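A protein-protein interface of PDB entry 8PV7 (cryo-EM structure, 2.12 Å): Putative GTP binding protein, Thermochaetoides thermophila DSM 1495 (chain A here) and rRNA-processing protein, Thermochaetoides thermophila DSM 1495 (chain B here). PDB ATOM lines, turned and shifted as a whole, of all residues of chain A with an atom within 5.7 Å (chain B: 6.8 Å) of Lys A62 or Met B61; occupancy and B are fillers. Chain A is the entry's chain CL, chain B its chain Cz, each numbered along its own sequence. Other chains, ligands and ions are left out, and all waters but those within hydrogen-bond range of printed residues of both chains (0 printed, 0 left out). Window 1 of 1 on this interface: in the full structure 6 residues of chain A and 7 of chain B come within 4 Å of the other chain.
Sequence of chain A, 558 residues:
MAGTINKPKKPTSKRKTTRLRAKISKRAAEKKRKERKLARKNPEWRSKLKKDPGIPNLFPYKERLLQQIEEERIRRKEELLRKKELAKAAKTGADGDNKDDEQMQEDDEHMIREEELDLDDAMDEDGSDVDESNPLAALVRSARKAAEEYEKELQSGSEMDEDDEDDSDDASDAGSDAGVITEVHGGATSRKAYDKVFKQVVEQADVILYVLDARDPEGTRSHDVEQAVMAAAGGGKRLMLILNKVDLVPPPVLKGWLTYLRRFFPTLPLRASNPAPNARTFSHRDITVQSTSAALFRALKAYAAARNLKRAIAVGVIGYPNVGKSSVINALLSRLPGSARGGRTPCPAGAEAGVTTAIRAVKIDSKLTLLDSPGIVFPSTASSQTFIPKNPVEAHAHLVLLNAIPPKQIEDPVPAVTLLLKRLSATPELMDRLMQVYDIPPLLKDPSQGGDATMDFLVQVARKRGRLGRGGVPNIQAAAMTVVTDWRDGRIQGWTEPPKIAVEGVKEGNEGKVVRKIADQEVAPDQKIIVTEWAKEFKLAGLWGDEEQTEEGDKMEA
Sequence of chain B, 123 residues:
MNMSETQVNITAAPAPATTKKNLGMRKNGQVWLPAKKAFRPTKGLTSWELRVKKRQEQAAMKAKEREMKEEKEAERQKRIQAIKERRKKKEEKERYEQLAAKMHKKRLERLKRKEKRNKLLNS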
ATOM      1  N   ILE A  55     -24.826  10.801  10.114  1.00  0.00           N
ATOM      2  CA  ILE A  55     -23.472  10.665   9.583  1.00  0.00           C
ATOM      3  C   ILE A  55     -22.917   9.315  10.024  1.00  0.00           C
ATOM      4  O   ILE A  55     -23.049   8.967  11.204  1.00  0.00           O
ATOM      5  CB  ILE A  55     -22.563  11.811  10.061  1.00  0.00           C
ATOM      6  CG1 ILE A  55     -23.267  13.155   9.880  1.00  0.00           C
ATOM      7  CG2 ILE A  55     -21.232  11.790   9.341  1.00  0.00           C
ATOM      8  CD1 ILE A  55     -22.633  14.269  10.652  1.00  0.00           C
ATOM      9  N   PRO A  56     -22.325   8.530   9.122  1.00  0.00           N
ATOM     10  CA  PRO A  56     -21.726   7.249   9.524  1.00  0.00           C
ATOM     11  C   PRO A  56     -20.573   7.447  10.497  1.00  0.00           C
ATOM     12  O   PRO A  56     -19.800   8.396  10.382  1.00  0.00           O
ATOM     13  CB  PRO A  56     -21.245   6.656   8.196  1.00  0.00           C
ATOM     14  CG  PRO A  56     -22.023   7.353   7.156  1.00  0.00           C
ATOM     15  CD  PRO A  56     -22.257   8.729   7.669  1.00  0.00           C
ATOM     16  N   ASN A  57     -20.462   6.522  11.453  1.00  0.00           N
ATOM     17  CA  ASN A  57     -19.430   6.619  12.481  1.00  0.00           C
ATOM     18  C   ASN A  57     -18.035   6.429  11.898  1.00  0.00           C
ATOM     19  O   ASN A  57     -17.068   7.021  12.385  1.00  0.00           O
ATOM     20  CB  ASN A  57     -19.687   5.589  13.580  1.00  0.00           C
ATOM     21  CG  ASN A  57     -20.959   5.856  14.348  1.00  0.00           C
ATOM     22  OD1 ASN A  57     -21.380   6.999  14.497  1.00  0.00           O
ATOM     23  ND2 ASN A  57     -21.580   4.796  14.841  1.00  0.00           N
ATOM     24  N   PHE A  59     -16.849   7.457   9.104  1.00  0.00           N
ATOM     25  CA  PHE A  59     -16.356   8.620   8.387  1.00  0.00           C
ATOM     26  C   PHE A  59     -15.324   9.348   9.244  1.00  0.00           C
ATOM     27  O   PHE A  59     -15.657   9.798  10.348  1.00  0.00           O
ATOM     28  CB  PHE A  59     -17.516   9.548   8.041  1.00  0.00           C
ATOM     29  CG  PHE A  59     -17.131  10.723   7.196  1.00  0.00           C
ATOM     30  CD1 PHE A  59     -16.579  10.541   5.944  1.00  0.00           C
ATOM     31  CD2 PHE A  59     -17.345  12.012   7.647  1.00  0.00           C
ATOM     32  CE1 PHE A  59     -16.233  11.622   5.165  1.00  0.00           C
ATOM     33  CE2 PHE A  59     -17.005  13.097   6.868  1.00  0.00           C
ATOM     34  CZ  PHE A  59     -16.448  12.900   5.625  1.00  0.00           C
ATOM     35  N   PRO A  60     -14.079   9.480   8.780  1.00  0.00           N
ATOM     36  CA  PRO A  60     -12.998   9.947   9.668  1.00  0.00           C
ATOM     37  C   PRO A  60     -13.125  11.388  10.122  1.00  0.00           C
ATOM     38  O   PRO A  60     -12.518  11.748  11.136  1.00  0.00           O
ATOM     39  CB  PRO A  60     -11.737   9.746   8.818  1.00  0.00           C
ATOM     40  CG  PRO A  60     -12.133   8.788   7.754  1.00  0.00           C
ATOM     41  CD  PRO A  60     -13.563   9.066   7.468  1.00  0.00           C
ATOM     42  N   TYR A  61     -13.880  12.227   9.417  1.00  0.00           N
ATOM     43  CA  TYR A  61     -14.006  13.636   9.772  1.00  0.00           C
ATOM     44  C   TYR A  61     -15.413  13.970  10.252  1.00  0.00           C
ATOM     45  O   TYR A  61     -15.901  15.090  10.065  1.00  0.00           O
ATOM     46  CB  TYR A  61     -13.594  14.517   8.595  1.00  0.00           C
ATOM     47  CG  TYR A  61     -12.241  14.143   8.036  1.00  0.00           C
ATOM     48  CD1 TYR A  61     -11.160  13.907   8.879  1.00  0.00           C
ATOM     49  CD2 TYR A  61     -12.045  14.015   6.672  1.00  0.00           C
ATOM     50  CE1 TYR A  61      -9.925  13.560   8.375  1.00  0.00           C
ATOM     51  CE2 TYR A  61     -10.816  13.669   6.159  1.00  0.00           C
ATOM     52  CZ  TYR A  61      -9.759  13.439   7.015  1.00  0.00           C
ATOM     53  OH  TYR A  61      -8.534  13.094   6.503  1.00  0.00           O
ATOM     54  N   LYS A  62     -16.064  12.993  10.887  1.00  0.00           N
ATOM     55  CA  LYS A  62     -17.404  13.201  11.423  1.00  0.00           C
ATOM     56  C   LYS A  62     -17.400  14.232  12.545  1.00  0.00           C
ATOM     57  O   LYS A  62     -18.314  15.057  12.639  1.00  0.00           O
ATOM     58  CB  LYS A  62     -17.981  11.870  11.903  1.00  0.00           C
ATOM     59  CG  LYS A  62     -19.333  11.990  12.566  1.00  0.00           C
ATOM     60  CD  LYS A  62     -19.973  10.645  12.795  1.00  0.00           C
ATOM     61  CE  LYS A  62     -21.288  10.789  13.530  1.00  0.00           C
ATOM     62  NZ  LYS A  62     -21.935   9.481  13.768  1.00  0.00           N
ATOM     63  N   GLU A  63     -16.377  14.207  13.400  1.00  0.00           N
ATOM     64  CA  GLU A  63     -16.289  15.186  14.480  1.00  0.00           C
ATOM     65  C   GLU A  63     -16.078  16.595  13.937  1.00  0.00           C
ATOM     66  O   GLU A  63     -16.653  17.560  14.452  1.00  0.00           O
ATOM     67  CB  GLU A  63     -15.175  14.803  15.453  1.00  0.00           C
ATOM     68  CG  GLU A  63     -15.128  15.666  16.697  1.00  0.00           C
ATOM     69  CD  GLU A  63     -14.699  14.903  17.932  1.00  0.00           C
ATOM     70  OE1 GLU A  63     -13.856  13.991  17.809  1.00  0.00           O
ATOM     71  OE2 GLU A  63     -15.202  15.218  19.030  1.00  0.00           O
ATOM     72  N   ARG A  64     -15.264  16.730  12.886  1.00  0.00           N
ATOM     73  CA  ARG A  64     -15.093  18.028  12.239  1.00  0.00           C
ATOM     74  C   ARG A  64     -16.392  18.510  11.603  1.00  0.00           C
ATOM     75  O   ARG A  64     -16.705  19.707  11.641  1.00  0.00           O
ATOM     76  CB  ARG A  64     -13.979  17.955  11.196  1.00  0.00           C
ATOM     77  CG  ARG A  64     -12.660  18.510  11.686  1.00  0.00           C
ATOM     78  CD  ARG A  64     -11.469  17.755  11.118  1.00  0.00           C
ATOM     79  NE  ARG A  64     -11.419  17.801   9.663  1.00  0.00           N
ATOM     80  CZ  ARG A  64     -10.377  17.416   8.941  1.00  0.00           C
ATOM     81  NH1 ARG A  64      -9.275  16.957   9.510  1.00  0.00           N
ATOM     82  NH2 ARG A  64     -10.439  17.496   7.616  1.00  0.00           N
ATOM     83  N   LEU A  65     -17.163  17.594  11.014  1.00  0.00           N
ATOM     84  CA  LEU A  65     -18.457  17.973  10.456  1.00  0.00           C
ATOM     85  C   LEU A  65     -19.428  18.416  11.549  1.00  0.00           C
ATOM     86  O   LEU A  65     -20.213  19.352  11.350  1.00  0.00           O
ATOM     87  CB  LEU A  65     -19.027  16.811   9.646  1.00  0.00           C
ATOM     88  CG  LEU A  65     -20.314  17.050   8.864  1.00  0.00           C
ATOM     89  CD1 LEU A  65     -20.220  18.329   8.050  1.00  0.00           C
ATOM     90  CD2 LEU A  65     -20.587  15.868   7.959  1.00  0.00           C
ATOM     91  N   LEU A  66     -19.382  17.761  12.710  1.00  0.00           N
ATOM     92  CA  LEU A  66     -20.207  18.185  13.840  1.00  0.00           C
ATOM     93  C   LEU A  66     -19.787  19.560  14.355  1.00  0.00           C
ATOM     94  O   LEU A  66     -20.640  20.377  14.732  1.00  0.00           O
ATOM     95  CB  LEU A  66     -20.143  17.144  14.955  1.00  0.00           C
ATOM     96  CG  LEU A  66     -20.765  15.782  14.641  1.00  0.00           C
ATOM     97  CD1 LEU A  66     -20.626  14.831  15.815  1.00  0.00           C
ATOM     98  CD2 LEU A  66     -22.218  15.922  14.230  1.00  0.00           C
ATOM     99  N   GLN A  67     -18.477  19.836  14.372  1.00  0.00           N
ATOM    100  CA  GLN A  67     -17.992  21.172  14.716  1.00  0.00           C
ATOM    101  C   GLN A  67     -18.508  22.221  13.741  1.00  0.00           C
ATOM    102  O   GLN A  67     -18.905  23.320  14.146  1.00  0.00           O
ATOM    103  CB  GLN A  67     -16.463  21.202  14.741  1.00  0.00           C
ATOM    104  CG  GLN A  67     -15.835  20.891  16.076  1.00  0.00           C
ATOM    105  CD  GLN A  67     -14.770  19.818  15.992  1.00  0.00           C
ATOM    106  OE1 GLN A  67     -14.030  19.735  15.013  1.00  0.00           O
ATOM    107  NE2 GLN A  67     -14.682  18.995  17.028  1.00  0.00           N
ATOM    108  N   GLN B  56     -10.091   6.384  21.706  1.00  0.00           N
ATOM    109  CA  GLN B  56     -10.329   7.625  22.444  1.00  0.00           C
ATOM    110  C   GLN B  56     -11.072   8.652  21.592  1.00  0.00           C
ATOM    111  O   GLN B  56     -12.049   9.268  22.049  1.00  0.00           O
ATOM    112  CB  GLN B  56      -9.002   8.194  22.941  1.00  0.00           C
ATOM    113  CG  GLN B  56      -8.456   7.492  24.160  1.00  0.00           C
ATOM    114  CD  GLN B  56      -6.961   7.677  24.321  1.00  0.00           C
ATOM    115  OE1 GLN B  56      -6.392   8.667  23.864  1.00  0.00           O
ATOM    116  NE2 GLN B  56      -6.316   6.719  24.973  1.00  0.00           N
ATOM    117  N   GLU B  57     -10.641   8.828  20.339  1.00  0.00           N
ATOM    118  CA  GLU B  57     -11.295   9.797  19.460  1.00  0.00           C
ATOM    119  C   GLU B  57     -12.734   9.401  19.139  1.00  0.00           C
ATOM    120  O   GLU B  57     -13.626  10.259  19.112  1.00  0.00           O
ATOM    121  CB  GLU B  57     -10.486   9.969  18.179  1.00  0.00           C
ATOM    122  CG  GLU B  57      -9.141  10.614  18.407  1.00  0.00           C
ATOM    123  CD  GLU B  57      -8.257  10.560  17.187  1.00  0.00           C
ATOM    124  OE1 GLU B  57      -8.636   9.892  16.204  1.00  0.00           O
ATOM    125  OE2 GLU B  57      -7.180  11.188  17.210  1.00  0.00           O
ATOM    126  N   GLN B  58     -12.980   8.110  18.893  1.00  0.00           N
ATOM    127  CA  GLN B  58     -14.332   7.649  18.599  1.00  0.00           C
ATOM    128  C   GLN B  58     -15.253   7.825  19.797  1.00  0.00           C
ATOM    129  O   GLN B  58     -16.416   8.209  19.633  1.00  0.00           O
ATOM    130  CB  GLN B  58     -14.314   6.189  18.153  1.00  0.00           C
ATOM    131  CG  GLN B  58     -13.961   5.986  16.692  1.00  0.00           C
ATOM    132  CD  GLN B  58     -14.999   6.562  15.748  1.00  0.00           C
ATOM    133  OE1 GLN B  58     -16.074   5.992  15.562  1.00  0.00           O
ATOM    134  NE2 GLN B  58     -14.683   7.701  15.149  1.00  0.00           N
ATOM    135  N   ALA B  59     -14.755   7.549  21.007  1.00  0.00           N
ATOM    136  CA  ALA B  59     -15.575   7.742  22.199  1.00  0.00           C
ATOM    137  C   ALA B  59     -15.922   9.212  22.408  1.00  0.00           C
ATOM    138  O   ALA B  59     -17.065   9.543  22.753  1.00  0.00           O
ATOM    139  CB  ALA B  59     -14.860   7.178  23.425  1.00  0.00           C
ATOM    140  N   ALA B  60     -14.952  10.110  22.195  1.00  0.00           N
ATOM    141  CA  ALA B  60     -15.225  11.539  22.335  1.00  0.00           C
ATOM    142  C   ALA B  60     -16.252  12.017  21.308  1.00  0.00           C
ATOM    143  O   ALA B  60     -17.184  12.764  21.642  1.00  0.00           O
ATOM    144  CB  ALA B  60     -13.925  12.331  22.211  1.00  0.00           C
ATOM    145  N   MET B  61     -16.108  11.566  20.056  1.00  0.00           N
ATOM    146  CA  MET B  61     -17.065  11.916  19.009  1.00  0.00           C
ATOM    147  C   MET B  61     -18.461  11.399  19.339  1.00  0.00           C
ATOM    148  O   MET B  61     -19.453  12.112  19.139  1.00  0.00           O
ATOM    149  CB  MET B  61     -16.539  11.390  17.661  1.00  0.00           C
ATOM    150  CG  MET B  61     -17.435  11.326  16.387  1.00  0.00           C
ATOM    151  SD  MET B  61     -19.001  10.414  16.312  1.00  0.00           S
ATOM    152  CE  MET B  61     -18.446   8.875  15.589  1.00  0.00           C
ATOM    153  N   LYS B  62     -18.561  10.163  19.837  1.00  0.00           N
ATOM    154  CA  LYS B  62     -19.875   9.603  20.141  1.00  0.00           C
ATOM    155  C   LYS B  62     -20.544  10.341  21.291  1.00  0.00           C
ATOM    156  O   LYS B  62     -21.756  10.585  21.255  1.00  0.00           O
ATOM    157  CB  LYS B  62     -19.768   8.109  20.455  1.00  0.00           C
ATOM    158  CG  LYS B  62     -19.481   7.211  19.253  1.00  0.00           C
ATOM    159  CD  LYS B  62     -20.724   6.490  18.741  1.00  0.00           C
ATOM    160  CE  LYS B  62     -21.578   7.385  17.856  1.00  0.00           C
ATOM    161  NZ  LYS B  62     -22.770   6.703  17.294  1.00  0.00           N
ATOM    162  N   ALA B  63     -19.769  10.711  22.317  1.00  0.00           N
ATOM    163  CA  ALA B  63     -20.327  11.478  23.428  1.00  0.00           C
ATOM    164  C   ALA B  63     -20.840  12.837  22.961  1.00  0.00           C
ATOM    165  O   ALA B  63     -21.926  13.283  23.362  1.00  0.00           O
ATOM    166  CB  ALA B  63     -19.274  11.644  24.523  1.00  0.00           C
ATOM    167  N   LYS B  64     -20.077  13.499  22.088  1.00  0.00           N
ATOM    168  CA  LYS B  64     -20.499  14.800  21.583  1.00  0.00           C
ATOM    169  C   LYS B  64     -21.767  14.698  20.732  1.00  0.00           C
ATOM    170  O   LYS B  64     -22.683  15.523  20.866  1.00  0.00           O
ATOM    171  CB  LYS B  64     -19.356  15.421  20.792  1.00  0.00           C
ATOM    172  CG  LYS B  64     -19.695  16.713  20.124  1.00  0.00           C
ATOM    173  CD  LYS B  64     -18.534  17.148  19.286  1.00  0.00           C
ATOM    174  CE  LYS B  64     -18.806  18.470  18.636  1.00  0.00           C
ATOM    175  NZ  LYS B  64     -17.625  18.890  17.877  1.00  0.00           N
ATOM    176  N   GLU B  65     -21.845  13.680  19.869  1.00  0.00           N
ATOM    177  CA  GLU B  65     -23.046  13.477  19.060  1.00  0.00           C
ATOM    178  C   GLU B  65     -24.254  13.158  19.934  1.00  0.00           C
ATOM    179  O   GLU B  65     -25.380  13.583  19.636  1.00  0.00           O
ATOM    180  CB  GLU B  65     -22.807  12.360  18.043  1.00  0.00           C
ATOM    181  CG  GLU B  65     -23.974  12.107  17.102  1.00  0.00           C
ATOM    182  CD  GLU B  65     -23.795  10.855  16.266  1.00  0.00           C
ATOM    183  OE1 GLU B  65     -22.851  10.089  16.539  1.00  0.00           O
ATOM    184  OE2 GLU B  65     -24.597  10.633  15.338  1.00  0.00           O
ATOM    185  N   ARG B  66     -24.034  12.420  21.028  1.00  0.00           N
ATOM    186  CA  ARG B  66     -25.109  12.144  21.973  1.00  0.00           C
ATOM    187  C   ARG B  66     -25.628  13.426  22.613  1.00  0.00           C
ATOM    188  O   ARG B  66     -26.841  13.587  22.794  1.00  0.00           O
ATOM    189  CB  ARG B  66     -24.628  11.169  23.044  1.00  0.00           C
ATOM    190  CG  ARG B  66     -25.470   9.920  23.160  1.00  0.00           C
ATOM    191  CD  ARG B  66     -24.673   8.772  23.751  1.00  0.00           C
ATOM    192  NE  ARG B  66     -23.657   9.234  24.688  1.00  0.00           N
ATOM    193  CZ  ARG B  66     -22.421   8.758  24.748  1.00  0.00           C
ATOM    194  NH1 ARG B  66     -22.004   7.812  23.924  1.00  0.00           N
ATOM    195  NH2 ARG B  66     -21.583   9.243  25.660  1.00  0.00           N
ATOM    196  N   LYS B  69     -27.833  15.221  20.021  1.00  0.00           N
ATOM    197  CA  LYS B  69     -29.134  14.586  19.851  1.00  0.00           C
ATOM    198  C   LYS B  69     -30.033  14.827  21.057  1.00  0.00           C
ATOM    199  O   LYS B  69     -31.247  15.006  20.903  1.00  0.00           O
ATOM    200  CB  LYS B  69     -28.960  13.094  19.589  1.00  0.00           C
ATOM    201  CG  LYS B  69     -28.430  12.779  18.206  1.00  0.00           C
ATOM    202  CD  LYS B  69     -28.247  11.288  18.025  1.00  0.00           C
ATOM    203  CE  LYS B  69     -27.957  10.935  16.580  1.00  0.00           C
ATOM    204  NZ  LYS B  69     -27.740   9.473  16.417  1.00  0.00           N
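Printed residues of chain A that touch a printed residue of chain B: Asn A57, Lys A62, Glu A63, Leu A66 and Gln A67.
Among the printed residues, 11 pairs touch across the chains.
The backbone carbonyl oxygen (O) of Ile A55 sits at hydrogen-bond distance from the side-chain amino group (NZ) of Lys A62 (2.8 Å).
The side-chain amide oxygen (OD1) of Asn A57 sits at hydrogen-bond distance from the side-chain amino group (NZ) of Lys A62, 2.6 Å away.
OE1 of Gln A67 sits close to O of Glu A63 (3.5 Å).
NZ of Lys B62 lies within salt-bridge range of OE1 of Glu B65, at 3.5 Å.
The side-chain carboxylate (OE2) of Glu B65 is in salt-bridge range of the side-chain amino group (NZ) of Lys B69 (3.5 Å).
OE1 of Gln B58 sits close to O of Asn A57 (3.5 Å).
OD1 of Asn A57 is in hydrogen-bond range of NZ of Lys B62 (3.1 Å).
NZ of Lys A62 lies within salt-bridge range of OE1 of Glu B65 (3.0 Å).
The side-chain amide nitrogen (NE2) of Gln A67 lies close to the side-chain amino group (NZ) of Lys B64.
Pro A56 touches none of the printed residues of chain B.
Phe A59 touches none of the printed residues of chain B.
Lys A62 touches two residues of chain B.
Printed residues of chain A within 4 Å of Glu B57: Glu A63 (3.96 Å).
Printed residues of chain A within 4 Å of Gln B58: Asn A57 (3.5 Å).
Met B61 touches just these residues of chain A: Asn A57, Lys A62 and Glu A63.
The nearest residue of chain B that does not touch Lys A62 is Lys B62 (4.6 Å).
The nearest residue of chain A that does not touch Met B61 is Leu A66 (4.5 Å).
The nearest printed residue of chain B that does not touch Glu A63 is Ala B60 (4.1 Å).
Among the printed residues, merely in contact across the chains: Lys A62 with Met B61, Asn A57 with Met B61, Glu A63 with Met B61, Glu A63 with Lys B64, Glu A63 with Glu B57, Leu A66 with Glu B65 and Asn A57 with Glu B65.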
